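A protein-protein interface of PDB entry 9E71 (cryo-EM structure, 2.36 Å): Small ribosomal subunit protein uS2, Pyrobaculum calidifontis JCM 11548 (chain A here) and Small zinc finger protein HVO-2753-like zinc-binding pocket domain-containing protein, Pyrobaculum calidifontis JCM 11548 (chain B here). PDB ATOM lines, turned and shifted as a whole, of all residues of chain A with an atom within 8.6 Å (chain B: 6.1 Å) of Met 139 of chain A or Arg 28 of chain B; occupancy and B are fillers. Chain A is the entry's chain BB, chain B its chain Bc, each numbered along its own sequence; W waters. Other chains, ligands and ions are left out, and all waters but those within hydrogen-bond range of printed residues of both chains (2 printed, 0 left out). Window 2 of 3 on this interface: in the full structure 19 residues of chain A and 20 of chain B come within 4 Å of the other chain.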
ATOM      1  N   GLY A 105       6.847 -13.124  25.146  1.00  0.00           N
ATOM      2  CA  GLY A 105       6.999 -14.269  26.010  1.00  0.00           C
ATOM      3  C   GLY A 105       5.980 -15.365  25.806  1.00  0.00           C
ATOM      4  O   GLY A 105       5.983 -16.337  26.569  1.00  0.00           O
ATOM      5  N   MET A 106       5.102 -15.243  24.808  1.00  0.00           N
ATOM      6  CA  MET A 106       4.146 -16.310  24.538  1.00  0.00           C
ATOM      7  C   MET A 106       4.850 -17.577  24.081  1.00  0.00           C
ATOM      8  O   MET A 106       4.426 -18.688  24.417  1.00  0.00           O
ATOM      9  CB  MET A 106       3.125 -15.864  23.496  1.00  0.00           C
ATOM     10  CG  MET A 106       1.733 -15.668  24.051  1.00  0.00           C
ATOM     11  SD  MET A 106       0.594 -15.028  22.816  1.00  0.00           S
ATOM     12  CE  MET A 106       0.967 -16.100  21.434  1.00  0.00           C
ATOM     13  N   LEU A 107       5.925 -17.436  23.311  1.00  0.00           N
ATOM     14  CA  LEU A 107       6.701 -18.590  22.885  1.00  0.00           C
ATOM     15  C   LEU A 107       7.937 -18.827  23.738  1.00  0.00           C
ATOM     16  O   LEU A 107       8.496 -19.928  23.697  1.00  0.00           O
ATOM     17  CB  LEU A 107       7.120 -18.435  21.422  1.00  0.00           C
ATOM     18  CG  LEU A 107       6.027 -17.980  20.454  1.00  0.00           C
ATOM     19  CD1 LEU A 107       6.527 -18.034  19.029  1.00  0.00           C
ATOM     20  CD2 LEU A 107       4.775 -18.821  20.611  1.00  0.00           C
ATOM     21  N   THR A 108       8.374 -17.834  24.512  1.00  0.00           N
ATOM     22  CA  THR A 108       9.597 -17.961  25.290  1.00  0.00           C
ATOM     23  C   THR A 108       9.356 -18.114  26.782  1.00  0.00           C
ATOM     24  O   THR A 108      10.228 -18.642  27.479  1.00  0.00           O
ATOM     25  CB  THR A 108      10.508 -16.750  25.069  1.00  0.00           C
ATOM     26  OG1 THR A 108      10.008 -15.639  25.818  1.00  0.00           O
ATOM     27  CG2 THR A 108      10.557 -16.384  23.601  1.00  0.00           C
ATOM     28  N   ASN A 109       8.212 -17.662  27.286  1.00  0.00           N
ATOM     29  CA  ASN A 109       7.895 -17.811  28.696  1.00  0.00           C
ATOM     30  C   ASN A 109       6.917 -18.957  28.853  1.00  0.00           C
ATOM     31  O   ASN A 109       5.715 -18.776  28.608  1.00  0.00           O
ATOM     32  CB  ASN A 109       7.303 -16.520  29.262  1.00  0.00           C
ATOM     33  CG  ASN A 109       7.118 -16.572  30.761  1.00  0.00           C
ATOM     34  OD1 ASN A 109       7.546 -17.517  31.425  1.00  0.00           O
ATOM     35  ND2 ASN A 109       6.470 -15.554  31.307  1.00  0.00           N
ATOM     36  N   PRO A 110       7.362 -20.143  29.269  1.00  0.00           N
ATOM     37  CA  PRO A 110       6.418 -21.248  29.492  1.00  0.00           C
ATOM     38  C   PRO A 110       5.515 -21.047  30.692  1.00  0.00           C
ATOM     39  O   PRO A 110       4.494 -21.739  30.791  1.00  0.00           O
ATOM     40  CB  PRO A 110       7.325 -22.471  29.680  1.00  0.00           C
ATOM     41  CG  PRO A 110       8.726 -21.987  29.632  1.00  0.00           C
ATOM     42  CD  PRO A 110       8.759 -20.507  29.542  1.00  0.00           C
ATOM     43  N   TYR A 115       0.848 -19.434  26.964  1.00  0.00           N
ATOM     44  CA  TYR A 115       2.071 -20.043  26.452  1.00  0.00           C
ATOM     45  C   TYR A 115       1.711 -21.096  25.417  1.00  0.00           C
ATOM     46  O   TYR A 115       1.329 -22.216  25.757  1.00  0.00           O
ATOM     47  CB  TYR A 115       2.883 -20.656  27.584  1.00  0.00           C
ATOM     48  CG  TYR A 115       4.039 -21.482  27.083  1.00  0.00           C
ATOM     49  CD1 TYR A 115       5.106 -20.889  26.428  1.00  0.00           C
ATOM     50  CD2 TYR A 115       4.061 -22.853  27.259  1.00  0.00           C
ATOM     51  CE1 TYR A 115       6.163 -21.637  25.969  1.00  0.00           C
ATOM     52  CE2 TYR A 115       5.114 -23.610  26.800  1.00  0.00           C
ATOM     53  CZ  TYR A 115       6.161 -22.996  26.156  1.00  0.00           C
ATOM     54  OH  TYR A 115       7.213 -23.751  25.699  1.00  0.00           O
ATOM     55  N   LEU A 116       1.838 -20.740  24.144  1.00  0.00           N
ATOM     56  CA  LEU A 116       1.545 -21.657  23.056  1.00  0.00           C
ATOM     57  C   LEU A 116       2.809 -22.395  22.650  1.00  0.00           C
ATOM     58  O   LEU A 116       3.920 -21.892  22.824  1.00  0.00           O
ATOM     59  CB  LEU A 116       0.979 -20.918  21.844  1.00  0.00           C
ATOM     60  CG  LEU A 116      -0.165 -19.915  21.996  1.00  0.00           C
ATOM     61  CD1 LEU A 116      -0.918 -19.807  20.685  1.00  0.00           C
ATOM     62  CD2 LEU A 116      -1.108 -20.294  23.124  1.00  0.00           C
ATOM     63  N   GLU A 117       2.630 -23.593  22.112  1.00  0.00           N
ATOM     64  CA  GLU A 117       3.715 -24.383  21.550  1.00  0.00           C
ATOM     65  C   GLU A 117       3.371 -24.652  20.092  1.00  0.00           C
ATOM     66  O   GLU A 117       2.378 -25.324  19.799  1.00  0.00           O
ATOM     67  CB  GLU A 117       3.905 -25.684  22.326  1.00  0.00           C
ATOM     68  CG  GLU A 117       4.574 -25.498  23.669  1.00  0.00           C
ATOM     69  CD  GLU A 117       6.033 -25.878  23.641  1.00  0.00           C
ATOM     70  OE1 GLU A 117       6.486 -26.409  22.607  1.00  0.00           O
ATOM     71  OE2 GLU A 117       6.731 -25.646  24.648  1.00  0.00           O
ATOM     72  N   VAL A 118       4.175 -24.118  19.180  1.00  0.00           N
ATOM     73  CA  VAL A 118       3.926 -24.284  17.758  1.00  0.00           C
ATOM     74  C   VAL A 118       5.217 -24.711  17.083  1.00  0.00           C
ATOM     75  O   VAL A 118       6.315 -24.535  17.612  1.00  0.00           O
ATOM     76  CB  VAL A 118       3.373 -23.004  17.098  1.00  0.00           C
ATOM     77  CG1 VAL A 118       2.254 -22.406  17.933  1.00  0.00           C
ATOM     78  CG2 VAL A 118       4.483 -21.995  16.885  1.00  0.00           C
ATOM     79  N   ASP A 119       5.067 -25.294  15.897  1.00  0.00           N
ATOM     80  CA  ASP A 119       6.198 -25.650  15.059  1.00  0.00           C
ATOM     81  C   ASP A 119       6.243 -24.877  13.753  1.00  0.00           C
ATOM     82  O   ASP A 119       7.134 -25.129  12.936  1.00  0.00           O
ATOM     83  CB  ASP A 119       6.185 -27.152  14.760  1.00  0.00           C
ATOM     84  CG  ASP A 119       5.810 -27.981  15.971  1.00  0.00           C
ATOM     85  OD1 ASP A 119       4.606 -28.050  16.295  1.00  0.00           O
ATOM     86  OD2 ASP A 119       6.719 -28.570  16.596  1.00  0.00           O
ATOM     87  N   ALA A 132       6.864 -11.343  17.120  1.00  0.00           N
ATOM     88  CA  ALA A 132       6.668 -12.745  16.781  1.00  0.00           C
ATOM     89  C   ALA A 132       7.877 -13.305  16.047  1.00  0.00           C
ATOM     90  O   ALA A 132       8.324 -14.422  16.335  1.00  0.00           O
ATOM     91  CB  ALA A 132       5.403 -12.907  15.940  1.00  0.00           C
ATOM     92  N   VAL A 133       8.427 -12.537  15.105  1.00  0.00           N
ATOM     93  CA  VAL A 133       9.609 -12.982  14.374  1.00  0.00           C
ATOM     94  C   VAL A 133      10.801 -13.106  15.311  1.00  0.00           C
ATOM     95  O   VAL A 133      11.623 -14.018  15.176  1.00  0.00           O
ATOM     96  CB  VAL A 133       9.909 -12.026  13.206  1.00  0.00           C
ATOM     97  CG1 VAL A 133      11.242 -12.379  12.565  1.00  0.00           C
ATOM     98  CG2 VAL A 133       8.788 -12.065  12.182  1.00  0.00           C
ATOM     99  N   ALA A 134      10.915 -12.189  16.275  1.00  0.00           N
ATOM    100  CA  ALA A 134      12.012 -12.253  17.234  1.00  0.00           C
ATOM    101  C   ALA A 134      11.918 -13.500  18.103  1.00  0.00           C
ATOM    102  O   ALA A 134      12.921 -14.188  18.334  1.00  0.00           O
ATOM    103  CB  ALA A 134      12.019 -10.999  18.102  1.00  0.00           C
ATOM    104  N   GLU A 135      10.716 -13.818  18.582  1.00  0.00           N
ATOM    105  CA  GLU A 135      10.562 -15.015  19.400  1.00  0.00           C
ATOM    106  C   GLU A 135      10.772 -16.277  18.574  1.00  0.00           C
ATOM    107  O   GLU A 135      11.330 -17.264  19.068  1.00  0.00           O
ATOM    108  CB  GLU A 135       9.193 -15.006  20.071  1.00  0.00           C
ATOM    109  CG  GLU A 135       9.137 -14.043  21.240  1.00  0.00           C
ATOM    110  CD  GLU A 135       7.899 -14.203  22.085  1.00  0.00           C
ATOM    111  OE1 GLU A 135       7.865 -15.126  22.925  1.00  0.00           O
ATOM    112  OE2 GLU A 135       6.970 -13.389  21.928  1.00  0.00           O
ATOM    113  N   ALA A 136      10.354 -16.257  17.307  1.00  0.00           N
ATOM    114  CA  ALA A 136      10.593 -17.396  16.429  1.00  0.00           C
ATOM    115  C   ALA A 136      12.081 -17.597  16.179  1.00  0.00           C
ATOM    116  O   ALA A 136      12.558 -18.735  16.120  1.00  0.00           O
ATOM    117  CB  ALA A 136       9.851 -17.207  15.109  1.00  0.00           C
ATOM    118  N   ALA A 137      12.829 -16.507  16.017  1.00  0.00           N
ATOM    119  CA  ALA A 137      14.276 -16.621  15.879  1.00  0.00           C
ATOM    120  C   ALA A 137      14.909 -17.167  17.151  1.00  0.00           C
ATOM    121  O   ALA A 137      15.816 -18.004  17.095  1.00  0.00           O
ATOM    122  CB  ALA A 137      14.881 -15.265  15.522  1.00  0.00           C
ATOM    123  N   LYS A 138      14.440 -16.705  18.310  1.00  0.00           N
ATOM    124  CA  LYS A 138      15.027 -17.153  19.566  1.00  0.00           C
ATOM    125  C   LYS A 138      14.737 -18.623  19.834  1.00  0.00           C
ATOM    126  O   LYS A 138      15.576 -19.324  20.412  1.00  0.00           O
ATOM    127  CB  LYS A 138      14.514 -16.296  20.720  1.00  0.00           C
ATOM    128  CG  LYS A 138      14.845 -16.854  22.088  1.00  0.00           C
ATOM    129  CD  LYS A 138      16.134 -16.266  22.630  1.00  0.00           C
ATOM    130  CE  LYS A 138      16.054 -16.063  24.133  1.00  0.00           C
ATOM    131  NZ  LYS A 138      16.879 -14.917  24.593  1.00  0.00           N
ATOM    132  N   MET A 139      13.567 -19.108  19.430  1.00  0.00           N
ATOM    133  CA  MET A 139      13.193 -20.482  19.739  1.00  0.00           C
ATOM    134  C   MET A 139      13.526 -21.475  18.636  1.00  0.00           C
ATOM    135  O   MET A 139      13.576 -22.680  18.898  1.00  0.00           O
ATOM    136  CB  MET A 139      11.700 -20.563  20.064  1.00  0.00           C
ATOM    137  CG  MET A 139      11.357 -19.977  21.411  1.00  0.00           C
ATOM    138  SD  MET A 139      12.107 -20.969  22.712  1.00  0.00           S
ATOM    139  CE  MET A 139      11.979 -19.867  24.108  1.00  0.00           C
ATOM    140  N   GLY A 140      13.753 -21.016  17.415  1.00  0.00           N
ATOM    141  CA  GLY A 140      14.006 -21.956  16.346  1.00  0.00           C
ATOM    142  C   GLY A 140      12.719 -22.539  15.810  1.00  0.00           C
ATOM    143  O   GLY A 140      12.567 -23.758  15.714  1.00  0.00           O
ATOM    144  N   ILE A 141      11.778 -21.665  15.469  1.00  0.00           N
ATOM    145  CA  ILE A 141      10.514 -22.044  14.856  1.00  0.00           C
ATOM    146  C   ILE A 141      10.540 -21.546  13.419  1.00  0.00           C
ATOM    147  O   ILE A 141      10.939 -20.406  13.181  1.00  0.00           O
ATOM    148  CB  ILE A 141       9.300 -21.459  15.599  1.00  0.00           C
ATOM    149  CG1 ILE A 141       9.309 -21.893  17.064  1.00  0.00           C
ATOM    150  CG2 ILE A 141       8.015 -21.870  14.914  1.00  0.00           C
ATOM    151  CD1 ILE A 141       9.198 -23.395  17.267  1.00  0.00           C
ATOM    152  N   PRO A 142      10.162 -22.364  12.440  1.00  0.00           N
ATOM    153  CA  PRO A 142      10.126 -21.889  11.050  1.00  0.00           C
ATOM    154  C   PRO A 142       9.121 -20.761  10.862  1.00  0.00           C
ATOM    155  O   PRO A 142       8.077 -20.715  11.514  1.00  0.00           O
ATOM    156  CB  PRO A 142       9.725 -23.132  10.247  1.00  0.00           C
ATOM    157  CG  PRO A 142       9.534 -24.233  11.222  1.00  0.00           C
ATOM    158  CD  PRO A 142       9.998 -23.819  12.562  1.00  0.00           C
ATOM    159  N   TYR A 155      15.577 -13.799   9.478  1.00  0.00           N
ATOM    160  CA  TYR A 155      14.874 -14.856  10.200  1.00  0.00           C
ATOM    161  C   TYR A 155      13.606 -15.326   9.506  1.00  0.00           C
ATOM    162  O   TYR A 155      12.714 -15.873  10.157  1.00  0.00           O
ATOM    163  CB  TYR A 155      14.529 -14.415  11.621  1.00  0.00           C
ATOM    164  CG  TYR A 155      15.727 -14.067  12.450  1.00  0.00           C
ATOM    165  CD1 TYR A 155      16.833 -14.893  12.482  1.00  0.00           C
ATOM    166  CD2 TYR A 155      15.746 -12.915  13.212  1.00  0.00           C
ATOM    167  CE1 TYR A 155      17.928 -14.578  13.248  1.00  0.00           C
ATOM    168  CE2 TYR A 155      16.832 -12.597  13.988  1.00  0.00           C
ATOM    169  CZ  TYR A 155      17.925 -13.424  13.995  1.00  0.00           C
ATOM    170  OH  TYR A 155      19.017 -13.096  14.763  1.00  0.00           O
ATOM    171  N   LEU B  23      24.715 -26.109  14.263  1.00  0.00           N
ATOM    172  CA  LEU B  23      23.772 -25.620  15.259  1.00  0.00           C
ATOM    173  C   LEU B  23      24.337 -25.902  16.642  1.00  0.00           C
ATOM    174  O   LEU B  23      24.169 -27.000  17.179  1.00  0.00           O
ATOM    175  CB  LEU B  23      22.397 -26.267  15.078  1.00  0.00           C
ATOM    176  CG  LEU B  23      21.681 -25.970  13.759  1.00  0.00           C
ATOM    177  CD1 LEU B  23      22.107 -26.935  12.682  1.00  0.00           C
ATOM    178  CD2 LEU B  23      20.182 -26.019  13.931  1.00  0.00           C
ATOM    179  N   ALA B  24      25.022 -24.921  17.218  1.00  0.00           N
ATOM    180  CA  ALA B  24      25.717 -25.122  18.473  1.00  0.00           C
ATOM    181  C   ALA B  24      24.733 -25.184  19.636  1.00  0.00           C
ATOM    182  O   ALA B  24      23.593 -24.730  19.525  1.00  0.00           O
ATOM    183  CB  ALA B  24      26.729 -24.003  18.700  1.00  0.00           C
ATOM    184  N   LEU B  26      22.755 -24.258  22.969  1.00  0.00           N
ATOM    185  CA  LEU B  26      22.184 -23.010  23.480  1.00  0.00           C
ATOM    186  C   LEU B  26      21.821 -22.025  22.373  1.00  0.00           C
ATOM    187  O   LEU B  26      21.251 -20.963  22.646  1.00  0.00           O
ATOM    188  CB  LEU B  26      23.118 -22.342  24.492  1.00  0.00           C
ATOM    189  CG  LEU B  26      23.560 -23.245  25.638  1.00  0.00           C
ATOM    190  CD1 LEU B  26      24.655 -22.583  26.452  1.00  0.00           C
ATOM    191  CD2 LEU B  26      22.368 -23.599  26.508  1.00  0.00           C
ATOM    192  N   GLU B  27      22.131 -22.364  21.126  1.00  0.00           N
ATOM    193  CA  GLU B  27      21.627 -21.616  19.989  1.00  0.00           C
ATOM    194  C   GLU B  27      20.729 -22.525  19.169  1.00  0.00           C
ATOM    195  O   GLU B  27      21.110 -23.648  18.827  1.00  0.00           O
ATOM    196  CB  GLU B  27      22.795 -21.086  19.150  1.00  0.00           C
ATOM    197  CG  GLU B  27      22.411 -20.321  17.884  1.00  0.00           C
ATOM    198  CD  GLU B  27      22.333 -21.213  16.655  1.00  0.00           C
ATOM    199  OE1 GLU B  27      21.213 -21.435  16.148  1.00  0.00           O
ATOM    200  OE2 GLU B  27      23.387 -21.710  16.211  1.00  0.00           O
ATOM    201  N   ARG B  28      19.535 -22.045  18.855  1.00  0.00           N
ATOM    202  CA  ARG B  28      18.536 -22.864  18.190  1.00  0.00           C
ATOM    203  C   ARG B  28      18.404 -22.439  16.739  1.00  0.00           C
ATOM    204  O   ARG B  28      17.960 -21.324  16.451  1.00  0.00           O
ATOM    205  CB  ARG B  28      17.186 -22.775  18.901  1.00  0.00           C
ATOM    206  CG  ARG B  28      17.005 -23.839  19.970  1.00  0.00           C
ATOM    207  CD  ARG B  28      15.791 -24.710  19.710  1.00  0.00           C
ATOM    208  NE  ARG B  28      15.916 -25.495  18.487  1.00  0.00           N
ATOM    209  CZ  ARG B  28      14.923 -26.170  17.926  1.00  0.00           C
ATOM    210  NH1 ARG B  28      13.706 -26.164  18.442  1.00  0.00           N
ATOM    211  NH2 ARG B  28      15.157 -26.872  16.822  1.00  0.00           N
ATOM    212  N   GLY B  29      18.796 -23.332  15.832  1.00  0.00           N
ATOM    213  CA  GLY B  29      18.532 -23.171  14.422  1.00  0.00           C
ATOM    214  C   GLY B  29      17.126 -23.618  14.071  1.00  0.00           C
ATOM    215  O   GLY B  29      16.209 -23.603  14.895  1.00  0.00           O
ATOM    216  N   VAL B  30      16.957 -24.021  12.820  1.00  0.00           N
ATOM    217  CA  VAL B  30      15.662 -24.471  12.336  1.00  0.00           C
ATOM    218  C   VAL B  30      15.858 -25.582  11.317  1.00  0.00           C
ATOM    219  O   VAL B  30      16.611 -25.431  10.351  1.00  0.00           O
ATOM    220  CB  VAL B  30      14.858 -23.304  11.736  1.00  0.00           C
ATOM    221  CG1 VAL B  30      13.810 -23.825  10.801  1.00  0.00           C
ATOM    222  CG2 VAL B  30      14.224 -22.505  12.844  1.00  0.00           C
ATOM    223  N   VAL B  31      15.166 -26.696  11.535  1.00  0.00           N
ATOM    224  CA  VAL B  31      15.191 -27.846  10.641  1.00  0.00           C
ATOM    225  C   VAL B  31      13.773 -28.066  10.145  1.00  0.00           C
ATOM    226  O   VAL B  31      12.836 -28.129  10.949  1.00  0.00           O
ATOM    227  CB  VAL B  31      15.709 -29.115  11.340  1.00  0.00           C
ATOM    228  CG1 VAL B  31      15.836 -30.246  10.337  1.00  0.00           C
ATOM    229  CG2 VAL B  31      17.028 -28.853  12.049  1.00  0.00           C
ATOM    230  N   ARG B  44      18.959 -24.748   8.804  1.00  0.00           N
ATOM    231  CA  ARG B  44      19.444 -23.377   8.805  1.00  0.00           C
ATOM    232  C   ARG B  44      19.897 -23.025  10.209  1.00  0.00           C
ATOM    233  O   ARG B  44      19.080 -22.990  11.134  1.00  0.00           O
ATOM    234  CB  ARG B  44      18.361 -22.403   8.339  1.00  0.00           C
ATOM    235  CG  ARG B  44      18.304 -22.217   6.844  1.00  0.00           C
ATOM    236  CD  ARG B  44      16.958 -21.692   6.395  1.00  0.00           C
ATOM    237  NE  ARG B  44      16.837 -20.242   6.515  1.00  0.00           N
ATOM    238  CZ  ARG B  44      17.516 -19.356   5.796  1.00  0.00           C
ATOM    239  NH1 ARG B  44      18.432 -19.729   4.919  1.00  0.00           N
ATOM    240  NH2 ARG B  44      17.266 -18.062   5.959  1.00  0.00           N
ATOM    241  N   SER B  45      21.188 -22.768  10.371  1.00  0.00           N
ATOM    242  CA  SER B  45      21.674 -22.232  11.629  1.00  0.00           C
ATOM    243  C   SER B  45      21.201 -20.793  11.787  1.00  0.00           C
ATOM    244  O   SER B  45      20.771 -20.152  10.828  1.00  0.00           O
ATOM    245  CB  SER B  45      23.197 -22.300  11.696  1.00  0.00           C
ATOM    246  OG  SER B  45      23.778 -21.408  10.766  1.00  0.00           O
ATOM    247  N   ALA B  46      21.282 -20.294  13.025  1.00  0.00           N
ATOM    248  CA  ALA B  46      20.772 -18.962  13.336  1.00  0.00           C
ATOM    249  C   ALA B  46      21.517 -17.880  12.567  1.00  0.00           C
ATOM    250  O   ALA B  46      20.927 -16.863  12.184  1.00  0.00           O
ATOM    251  CB  ALA B  46      20.864 -18.705  14.838  1.00  0.00           C
ATOM    252  N   ARG B  49      20.008 -17.916   9.121  1.00  0.00           N
ATOM    253  CA  ARG B  49      18.654 -17.375   9.186  1.00  0.00           C
ATOM    254  C   ARG B  49      18.674 -15.856   9.285  1.00  0.00           C
ATOM    255  O   ARG B  49      17.899 -15.170   8.610  1.00  0.00           O
ATOM    256  CB  ARG B  49      17.893 -17.991  10.362  1.00  0.00           C
ATOM    257  CG  ARG B  49      17.901 -19.505  10.351  1.00  0.00           C
ATOM    258  CD  ARG B  49      17.513 -20.126  11.687  1.00  0.00           C
ATOM    259  NE  ARG B  49      16.493 -19.381  12.413  1.00  0.00           N
ATOM    260  CZ  ARG B  49      15.210 -19.369  12.087  1.00  0.00           C
ATOM    261  NH1 ARG B  49      14.772 -19.984  11.007  1.00  0.00           N
ATOM    262  NH2 ARG B  49      14.348 -18.728  12.866  1.00  0.00           N
HETATM  263  O   HOH W   1      17.635 -18.894  14.741  1.00  0.00           O
HETATM  264  O   HOH W   2      19.005 -19.435  20.000  1.00  0.00           O
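The backbone NH (N) of Tyr 155 of chain A lies within hydrogen-bond range of the backbone carbonyl oxygen (O) of Arg 49 of chain B, 2.8 Å away.
The backbone NH (N) of Ile 141 of chain A is in hydrogen-bond range of the backbone carbonyl oxygen (O) of Ala 136 of chain A (3.1 Å). The side-chain carboxylate of Glu 27 of chain B lies within hydrogen-bond range of the backbone NH of Gly 29 of chain B. The side-chain carboxylate of Glu 27 of chain B lies close to the backbone NH of Ala 46 of chain B (3.3 Å). N of Arg 44 of chain B is in hydrogen-bond range of O of Val 30 of chain B, at 2.9 Å.
Among the printed residues, merely in contact across the chains: Ala 136 of chain A with Arg 49 of chain B, Ala 137 of chain A with Arg 49 of chain B, Met 139 of chain A with Arg 28 of chain B, Gly 140 of chain A with Arg 28 of chain B, Gly 140 of chain A with Gly 29 of chain B, Gly 140 of chain A with Val 30 of chain B, Ile 141 of chain A with Val 30 of chain B, Ile 141 of chain A with Arg 49 of chain B and Tyr 155 of chain A with Ala 46 of chain B.
Printed residues of chain B within 4 Å of Ala 137 of chain A: Arg 49 (3.7 Å). Met 139 of chain A touches one residue of chain B. Of the printed residues of chain B, Gly 140 of chain A touches Arg 28 (3.8 Å), Gly 29 (3.1 Å) and Val 30 (3.3 Å). Of the printed residues of chain B, Ile 141 of chain A touches Val 30 (3.7 Å) and Arg 49 (3.8 Å). Of the printed residues of chain B, Tyr 155 of chain A touches Ala 46 and Arg 49.
Printed residues of chain A that touch a printed residue of chain B: Ala 136, Ala 137, Met 139, Gly 140, Ile 141 and Tyr 155. Hydrophobic or aromatic side chains of chain A within 4 Å of the printed part of chain B: Tyr 155. Of the 12 printed residues of chain B, 5 touch a printed residue of chain A. Hydrophobic or aromatic side chains of chain B within 4 Å of the printed part of chain A: Val 30. Among the printed residues, no Asp or Glu carboxylate lies within 4 Å of a Lys or Arg side-chain nitrogen of the other chain.
Water W1 lies within hydrogen-bond range of NE of Arg 49 of chain B (2.6 Å), O of Arg 28 of chain B (3.0 Å) and O of Ala 137 of chain A (3.1 Å). Water W2 bridges N of Arg 28 of chain B and O of Lys 138 of chain A.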
